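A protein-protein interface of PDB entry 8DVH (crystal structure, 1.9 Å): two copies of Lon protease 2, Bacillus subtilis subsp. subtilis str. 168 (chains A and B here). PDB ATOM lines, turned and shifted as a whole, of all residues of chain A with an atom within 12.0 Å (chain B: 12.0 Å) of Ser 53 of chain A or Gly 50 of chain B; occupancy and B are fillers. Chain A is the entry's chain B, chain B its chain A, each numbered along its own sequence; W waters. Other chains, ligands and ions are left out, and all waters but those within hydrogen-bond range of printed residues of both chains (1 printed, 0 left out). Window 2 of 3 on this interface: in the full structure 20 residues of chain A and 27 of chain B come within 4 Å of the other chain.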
ATOM      1  N   SER A  48      17.725  -3.095  16.344  1.00  0.00           N
ATOM      2  CA  SER A  48      17.727  -2.391  15.059  1.00  0.00           C
ATOM      3  C   SER A  48      18.107  -0.937  15.327  1.00  0.00           C
ATOM      4  O   SER A  48      17.584  -0.372  16.312  1.00  0.00           O
ATOM      5  CB  SER A  48      16.388  -2.446  14.367  1.00  0.00           C
ATOM      6  OG  SER A  48      16.051  -3.790  14.078  1.00  0.00           O
ATOM      7  N   ILE A  49      19.018  -0.419  14.516  1.00  0.00           N
ATOM      8  CA  ILE A  49      19.474   0.992  14.520  1.00  0.00           C
ATOM      9  C   ILE A  49      19.245   1.531  13.127  1.00  0.00           C
ATOM     10  O   ILE A  49      19.713   0.914  12.160  1.00  0.00           O
ATOM     11  CB  ILE A  49      20.948   1.068  14.940  1.00  0.00           C
ATOM     12  CG1 ILE A  49      21.097   0.510  16.358  1.00  0.00           C
ATOM     13  CG2 ILE A  49      21.475   2.483  14.781  1.00  0.00           C
ATOM     14  CD1 ILE A  49      22.499   0.451  16.875  1.00  0.00           C
ATOM     15  N   GLY A  50      18.592   2.679  13.044  1.00  0.00           N
ATOM     16  CA  GLY A  50      18.285   3.192  11.709  1.00  0.00           C
ATOM     17  C   GLY A  50      18.294   4.692  11.579  1.00  0.00           C
ATOM     18  O   GLY A  50      18.297   5.387  12.573  1.00  0.00           O
ATOM     19  N   SER A  51      18.365   5.100  10.324  1.00  0.00           N
ATOM     20  CA  SER A  51      18.341   6.488   9.818  1.00  0.00           C
ATOM     21  C   SER A  51      17.003   6.676   9.110  1.00  0.00           C
ATOM     22  O   SER A  51      16.054   5.955   9.411  1.00  0.00           O
ATOM     23  CB  SER A  51      19.421   6.625   8.800  1.00  0.00           C
ATOM     24  OG  SER A  51      20.628   6.073   9.281  1.00  0.00           O
ATOM     25  N   GLN A  52      16.940   7.672   8.244  1.00  0.00           N
ATOM     26  CA  GLN A  52      15.792   7.883   7.321  1.00  0.00           C
ATOM     27  C   GLN A  52      15.702   6.690   6.365  1.00  0.00           C
ATOM     28  O   GLN A  52      14.631   6.062   6.299  1.00  0.00           O
ATOM     29  CB  GLN A  52      15.927   9.181   6.512  1.00  0.00           C
ATOM     30  CG  GLN A  52      14.987   9.233   5.310  1.00  0.00           C
ATOM     31  CD  GLN A  52      14.637  10.629   4.844  1.00  0.00           C
ATOM     32  OE1 GLN A  52      15.472  11.531   4.825  1.00  0.00           O
ATOM     33  NE2 GLN A  52      13.389  10.810   4.433  1.00  0.00           N
ATOM     34  N   SER A  53      16.789   6.385   5.657  1.00  0.00           N
ATOM     35  CA  SER A  53      16.743   5.509   4.461  1.00  0.00           C
ATOM     36  C   SER A  53      17.531   4.201   4.668  1.00  0.00           C
ATOM     37  O   SER A  53      17.692   3.457   3.698  1.00  0.00           O
ATOM     38  CB  SER A  53      17.199   6.307   3.243  1.00  0.00           C
ATOM     39  OG  SER A  53      18.580   6.097   2.991  1.00  0.00           O
ATOM     40  N   LYS A  54      18.038   3.935   5.874  1.00  0.00           N
ATOM     41  CA  LYS A  54      18.929   2.764   6.100  1.00  0.00           C
ATOM     42  C   LYS A  54      18.783   2.266   7.528  1.00  0.00           C
ATOM     43  O   LYS A  54      18.662   3.076   8.455  1.00  0.00           O
ATOM     44  CB  LYS A  54      20.358   3.192   5.769  1.00  0.00           C
ATOM     45  CG  LYS A  54      21.467   2.190   6.003  1.00  0.00           C
ATOM     46  CD  LYS A  54      22.821   2.710   5.491  1.00  0.00           C
ATOM     47  CE  LYS A  54      22.750   3.278   4.084  1.00  0.00           C
ATOM     48  NZ  LYS A  54      24.084   3.511   3.464  1.00  0.00           N
ATOM     49  N   SER A  55      18.874   0.948   7.732  1.00  0.00           N
ATOM     50  CA  SER A  55      18.856   0.408   9.089  1.00  0.00           C
ATOM     51  C   SER A  55      19.563  -0.927   9.112  1.00  0.00           C
ATOM     52  O   SER A  55      19.702  -1.580   8.049  1.00  0.00           O
ATOM     53  CB  SER A  55      17.459   0.312   9.616  1.00  0.00           C
ATOM     54  OG  SER A  55      16.767  -0.697   8.960  1.00  0.00           O
ATOM     55  N   ILE A  56      20.086  -1.247  10.270  1.00  0.00           N
ATOM     56  CA  ILE A  56      20.739  -2.559  10.427  1.00  0.00           C
ATOM     57  C   ILE A  56      20.075  -3.251  11.606  1.00  0.00           C
ATOM     58  O   ILE A  56      19.566  -2.589  12.571  1.00  0.00           O
ATOM     59  CB  ILE A  56      22.263  -2.447  10.561  1.00  0.00           C
ATOM     60  CG1 ILE A  56      22.655  -1.674  11.799  1.00  0.00           C
ATOM     61  CG2 ILE A  56      22.950  -1.884   9.304  1.00  0.00           C
ATOM     62  CD1 ILE A  56      23.714  -2.389  12.539  1.00  0.00           C
ATOM     63  N   ARG A  57      20.200  -4.563  11.572  1.00  0.00           N
ATOM     64  CA  ARG A  57      19.621  -5.450  12.581  1.00  0.00           C
ATOM     65  C   ARG A  57      20.711  -6.435  12.984  1.00  0.00           C
ATOM     66  O   ARG A  57      21.453  -6.820  12.125  1.00  0.00           O
ATOM     67  CB  ARG A  57      18.510  -6.214  11.868  1.00  0.00           C
ATOM     68  CG  ARG A  57      17.548  -6.975  12.754  1.00  0.00           C
ATOM     69  CD  ARG A  57      16.363  -7.391  11.909  1.00  0.00           C
ATOM     70  NE  ARG A  57      16.227  -8.822  12.069  1.00  0.00           N
ATOM     71  CZ  ARG A  57      15.709  -9.658  11.187  1.00  0.00           C
ATOM     72  NH1 ARG A  57      15.256  -9.211  10.034  1.00  0.00           N
ATOM     73  NH2 ARG A  57      15.653 -10.944  11.466  1.00  0.00           N
ATOM     74  N   GLU B  46      22.172  -7.745   9.135  1.00  0.00           N
ATOM     75  CA  GLU B  46      21.291  -7.495   7.975  1.00  0.00           C
ATOM     76  C   GLU B  46      21.176  -5.985   7.834  1.00  0.00           C
ATOM     77  O   GLU B  46      21.198  -5.324   8.860  1.00  0.00           O
ATOM     78  CB  GLU B  46      19.969  -8.192   8.285  1.00  0.00           C
ATOM     79  CG  GLU B  46      18.825  -7.932   7.375  1.00  0.00           C
ATOM     80  CD  GLU B  46      17.544  -8.385   8.095  1.00  0.00           C
ATOM     81  OE1 GLU B  46      17.490  -9.555   8.533  1.00  0.00           O
ATOM     82  OE2 GLU B  46      16.727  -7.547   8.379  1.00  0.00           O
ATOM     83  N   GLU B  47      21.008  -5.507   6.611  1.00  0.00           N
ATOM     84  CA  GLU B  47      20.847  -4.055   6.330  1.00  0.00           C
ATOM     85  C   GLU B  47      19.613  -3.913   5.457  1.00  0.00           C
ATOM     86  O   GLU B  47      19.419  -4.756   4.601  1.00  0.00           O
ATOM     87  CB  GLU B  47      22.124  -3.567   5.636  1.00  0.00           C
ATOM     88  CG  GLU B  47      22.151  -2.092   5.386  1.00  0.00           C
ATOM     89  CD  GLU B  47      23.378  -1.638   4.609  1.00  0.00           C
ATOM     90  OE1 GLU B  47      24.001  -2.454   3.927  1.00  0.00           O
ATOM     91  OE2 GLU B  47      23.621  -0.429   4.608  1.00  0.00           O
ATOM     92  N   SER B  48      18.772  -2.927   5.751  1.00  0.00           N
ATOM     93  CA  SER B  48      17.633  -2.514   4.929  1.00  0.00           C
ATOM     94  C   SER B  48      17.944  -1.124   4.397  1.00  0.00           C
ATOM     95  O   SER B  48      18.497  -0.310   5.164  1.00  0.00           O
ATOM     96  CB  SER B  48      16.347  -2.536   5.715  1.00  0.00           C
ATOM     97  OG  SER B  48      16.129  -3.886   6.097  1.00  0.00           O
ATOM     98  N   ILE B  49      17.753  -0.941   3.094  1.00  0.00           N
ATOM     99  CA  ILE B  49      17.997   0.362   2.423  1.00  0.00           C
ATOM    100  C   ILE B  49      16.765   0.739   1.601  1.00  0.00           C
ATOM    101  O   ILE B  49      16.308  -0.081   0.781  1.00  0.00           O
ATOM    102  CB  ILE B  49      19.230   0.245   1.532  1.00  0.00           C
ATOM    103  CG1 ILE B  49      20.454  -0.205   2.329  1.00  0.00           C
ATOM    104  CG2 ILE B  49      19.436   1.559   0.779  1.00  0.00           C
ATOM    105  CD1 ILE B  49      21.584  -0.778   1.506  1.00  0.00           C
ATOM    106  N   GLY B  50      16.296   1.976   1.733  1.00  0.00           N
ATOM    107  CA  GLY B  50      15.297   2.507   0.803  1.00  0.00           C
ATOM    108  C   GLY B  50      14.243   3.264   1.561  1.00  0.00           C
ATOM    109  O   GLY B  50      14.598   3.968   2.495  1.00  0.00           O
ATOM    110  N   SER B  51      12.997   3.131   1.145  1.00  0.00           N
ATOM    111  CA  SER B  51      11.826   3.813   1.732  1.00  0.00           C
ATOM    112  C   SER B  51      10.641   2.849   1.741  1.00  0.00           C
ATOM    113  O   SER B  51      10.751   1.740   1.193  1.00  0.00           O
ATOM    114  CB  SER B  51      11.492   5.028   0.910  1.00  0.00           C
ATOM    115  OG  SER B  51      11.204   4.632  -0.427  1.00  0.00           O
ATOM    116  N   GLN B  52       9.503   3.351   2.214  1.00  0.00           N
ATOM    117  CA  GLN B  52       8.167   2.724   2.083  1.00  0.00           C
ATOM    118  C   GLN B  52       7.997   2.233   0.639  1.00  0.00           C
ATOM    119  O   GLN B  52       7.669   1.019   0.466  1.00  0.00           O
ATOM    120  CB  GLN B  52       7.112   3.747   2.509  1.00  0.00           C
ATOM    121  CG  GLN B  52       5.668   3.360   2.226  1.00  0.00           C
ATOM    122  CD  GLN B  52       4.742   4.463   2.684  1.00  0.00           C
ATOM    123  OE1 GLN B  52       4.567   4.679   3.883  1.00  0.00           O
ATOM    124  NE2 GLN B  52       4.159   5.187   1.733  1.00  0.00           N
ATOM    125  N   SER B  53       8.259   3.088  -0.361  1.00  0.00           N
ATOM    126  CA  SER B  53       7.846   2.809  -1.761  1.00  0.00           C
ATOM    127  C   SER B  53       8.662   1.639  -2.319  1.00  0.00           C
ATOM    128  O   SER B  53       8.046   0.777  -2.961  1.00  0.00           O
ATOM    129  CB  SER B  53       7.871   4.022  -2.666  1.00  0.00           C
ATOM    130  OG  SER B  53       9.184   4.468  -2.924  1.00  0.00           O
ATOM    131  N   LYS B  54       9.974   1.607  -2.094  1.00  0.00           N
ATOM    132  CA  LYS B  54      10.819   0.432  -2.436  1.00  0.00           C
ATOM    133  C   LYS B  54      12.012   0.354  -1.477  1.00  0.00           C
ATOM    134  O   LYS B  54      12.728   1.373  -1.273  1.00  0.00           O
ATOM    135  CB  LYS B  54      11.291   0.510  -3.895  1.00  0.00           C
ATOM    136  CG  LYS B  54      11.901  -0.790  -4.405  1.00  0.00           C
ATOM    137  CD  LYS B  54      12.399  -0.741  -5.861  1.00  0.00           C
ATOM    138  CE  LYS B  54      11.258  -0.626  -6.862  1.00  0.00           C
ATOM    139  NZ  LYS B  54      11.606  -1.249  -8.163  1.00  0.00           N
ATOM    140  N   SER B  55      12.247  -0.814  -0.896  1.00  0.00           N
ATOM    141  CA  SER B  55      13.436  -1.036  -0.067  1.00  0.00           C
ATOM    142  C   SER B  55      13.925  -2.443  -0.356  1.00  0.00           C
ATOM    143  O   SER B  55      13.121  -3.256  -0.882  1.00  0.00           O
ATOM    144  CB  SER B  55      13.146  -0.800   1.391  1.00  0.00           C
ATOM    145  OG  SER B  55      12.275  -1.791   1.899  1.00  0.00           O
ATOM    146  N   ILE B  56      15.187  -2.675  -0.059  1.00  0.00           N
ATOM    147  CA  ILE B  56      15.797  -4.012  -0.151  1.00  0.00           C
ATOM    148  C   ILE B  56      16.333  -4.357   1.221  1.00  0.00           C
ATOM    149  O   ILE B  56      16.620  -3.451   2.047  1.00  0.00           O
ATOM    150  CB  ILE B  56      16.889  -4.063  -1.231  1.00  0.00           C
ATOM    151  CG1 ILE B  56      17.960  -2.994  -1.014  1.00  0.00           C
ATOM    152  CG2 ILE B  56      16.296  -3.989  -2.631  1.00  0.00           C
ATOM    153  CD1 ILE B  56      19.236  -3.311  -1.688  1.00  0.00           C
ATOM    154  N   ARG B  57      16.540  -5.639   1.417  1.00  0.00           N
ATOM    155  CA  ARG B  57      17.161  -6.153   2.619  1.00  0.00           C
ATOM    156  C   ARG B  57      18.259  -7.083   2.141  1.00  0.00           C
ATOM    157  O   ARG B  57      18.008  -7.795   1.142  1.00  0.00           O
ATOM    158  CB  ARG B  57      16.116  -6.944   3.393  1.00  0.00           C
ATOM    159  CG  ARG B  57      16.320  -6.955   4.884  1.00  0.00           C
ATOM    160  CD  ARG B  57      14.987  -7.399   5.505  1.00  0.00           C
ATOM    161  NE  ARG B  57      15.205  -8.749   5.959  1.00  0.00           N
ATOM    162  CZ  ARG B  57      14.289  -9.645   6.286  1.00  0.00           C
ATOM    163  NH1 ARG B  57      12.999  -9.402   6.121  1.00  0.00           N
ATOM    164  NH2 ARG B  57      14.696 -10.812   6.734  1.00  0.00           N
ATOM    165  N   ARG B  58      19.391  -7.060   2.833  1.00  0.00           N
ATOM    166  CA  ARG B  58      20.467  -8.005   2.492  1.00  0.00           C
ATOM    167  C   ARG B  58      21.244  -8.396   3.726  1.00  0.00           C
ATOM    168  O   ARG B  58      21.184  -7.686   4.782  1.00  0.00           O
ATOM    169  CB  ARG B  58      21.383  -7.346   1.465  1.00  0.00           C
ATOM    170  CG  ARG B  58      22.055  -6.100   1.964  1.00  0.00           C
ATOM    171  CD  ARG B  58      23.316  -5.966   1.155  1.00  0.00           C
ATOM    172  NE  ARG B  58      24.028  -4.720   1.376  1.00  0.00           N
ATOM    173  CZ  ARG B  58      25.175  -4.427   0.758  1.00  0.00           C
ATOM    174  NH1 ARG B  58      25.718  -5.294  -0.091  1.00  0.00           N
ATOM    175  NH2 ARG B  58      25.740  -3.256   0.981  1.00  0.00           N
ATOM    176  N   MET B  61      27.311  -6.421   4.922  1.00  0.00           N
ATOM    177  CA  MET B  61      28.684  -6.518   4.345  1.00  0.00           C
ATOM    178  C   MET B  61      29.592  -7.321   5.265  1.00  0.00           C
ATOM    179  O   MET B  61      30.382  -8.151   4.754  1.00  0.00           O
ATOM    180  CB  MET B  61      29.224  -5.107   4.150  1.00  0.00           C
ATOM    181  CG  MET B  61      28.508  -4.393   3.033  1.00  0.00           C
ATOM    182  SD  MET B  61      29.010  -2.688   2.904  1.00  0.00           S
ATOM    183  CE  MET B  61      28.113  -1.980   4.281  1.00  0.00           C
ATOM    184  N   ASP B  96      30.080  -2.875  10.830  1.00  0.00           N
ATOM    185  CA  ASP B  96      29.689  -3.387   9.500  1.00  0.00           C
ATOM    186  C   ASP B  96      30.806  -3.083   8.514  1.00  0.00           C
ATOM    187  O   ASP B  96      31.646  -2.233   8.823  1.00  0.00           O
ATOM    188  CB  ASP B  96      28.406  -2.732   9.011  1.00  0.00           C
ATOM    189  CG  ASP B  96      27.620  -3.565   8.023  1.00  0.00           C
ATOM    190  OD1 ASP B  96      28.109  -4.706   7.644  1.00  0.00           O
ATOM    191  OD2 ASP B  96      26.509  -3.068   7.647  1.00  0.00           O
HETATM  192  O   HOH W   1      25.420   0.775   3.427  1.00  0.00           O
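The backbone NH of Ser 48 of chain B is in hydrogen-bond range of the backbone carbonyl oxygen of Ser 55 of chain A, at 2.8 Å. OE1 of Glu 46 of chain B is in salt-bridge range of NH1 of Arg 57 of chain A (2.7 Å). The backbone carbonyl oxygen (O) of Ser 53 of chain A is in hydrogen-bond range of the backbone NH (N) of Gly 50 of chain B, at 2.8 Å.
The backbone NH (N) of Ile 49 of chain B sits at hydrogen-bond distance from the backbone carbonyl oxygen (O) of Ile 56 of chain B. The guanidinium group of Arg 58 of chain B is in salt-bridge range of the side-chain carboxylate of Glu 47 of chain B. The guanidinium group (NE) of Arg 57 of chain B is in salt-bridge range of the side-chain carboxylate (OE2) of Glu 46 of chain B (3.1 Å). O of Ile 49 of chain A sits at hydrogen-bond distance from N of Ile 56 of chain A (2.9 Å).
Among the printed residues, merely in contact across the chains: Ser 53 of chain A with Ile 49 of chain B (3.4 Å), Lys 54 of chain A with Glu 47 of chain B (3.4 Å), Lys 54 of chain A with Ser 48 of chain B (3.2 Å), Ser 55 of chain A with Glu 47 of chain B (3.2 Å), Ile 56 of chain A with Glu 46 of chain B (3.2 Å) and Arg 57 of chain A with Arg 57 of chain B (3.7 Å).
Ser 53 of chain A touches just these residues of chain B: Ile 49 (3.4 Å) and Gly 50 (2.8 Å). Gly 50 of chain B touches one residue of chain A. No residue of chain B comes within 4 Å of Ser 51 of chain A. Lys 54 of chain A touches just these residues of chain B: Glu 47 (3.4 Å) and Ser 48 (3.2 Å). Of chain B, only Glu 47 (3.2 Å) and Ser 48 (2.8 Å) come within 4 Å of Ser 55 of chain A. Of chain A, only Lys 54 and Ser 55 come within 4 Å of Ser 48 of chain B. Ile 49 of chain B touches just one residue of chain A: Ser 53. No residue of chain A comes within 4 Å of Ser 51 of chain B. No residue of chain A comes within 4 Å of Ile 56 of chain B. Printed residues of chain B within 4 Å of Arg 57 of chain A: Glu 46 and Arg 57. Printed residues of chain A within 4 Å of Glu 47 of chain B: Lys 54 (3.4 Å) and Ser 55 (3.2 Å). Of the printed residues of chain A, Arg 57 of chain B touches Arg 57 (3.7 Å). Of the printed residues of chain A, Glu 46 of chain B touches Ile 56 and Arg 57. Of the printed residues of chain B, Ile 56 of chain A touches Glu 46 (3.2 Å). Ser 53 of chain B touches none of the printed residues of chain A. Met 61 of chain B touches none of the printed residues of chain A. The nearest residue of chain A that does not touch Gly 50 of chain B is Gln 52 of chain A (4.3 Å). The nearest printed residue of chain A that does not touch Glu 46 of chain B is Ser 55 of chain A (4.1 Å).
Along chain A the printed residues that touch a printed residue of chain B span positions 53 to 57.
Ser 53 of chain A touches Ile 49 of chain B, but with the chains exchanged Ile 49 of chain A does not touch Ser 53 of chain B (17.1 Å). Ser 53 of chain A touches Gly 50 of chain B, but with the chains exchanged Gly 50 of chain A does not touch Ser 53 of chain B (15.7 Å). Ser 55 of chain A touches Ser 48 of chain B, but with the chains exchanged Ser 48 of chain A does not touch Ser 55 of chain B (12.9 Å). Arg 57 of chain B touches its own counterpart, Arg 57 of chain A. Of the 9 pairs that touch across the chains among the printed residues, 1 has its exchanged pair printed and touching as well.
Water W1 lies within hydrogen-bond range of the side-chain carboxylate (OE2) of Glu 47 of chain B (2.5 Å) and the side-chain amino group (NZ) of Lys 54 of chain A (3.0 Å).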
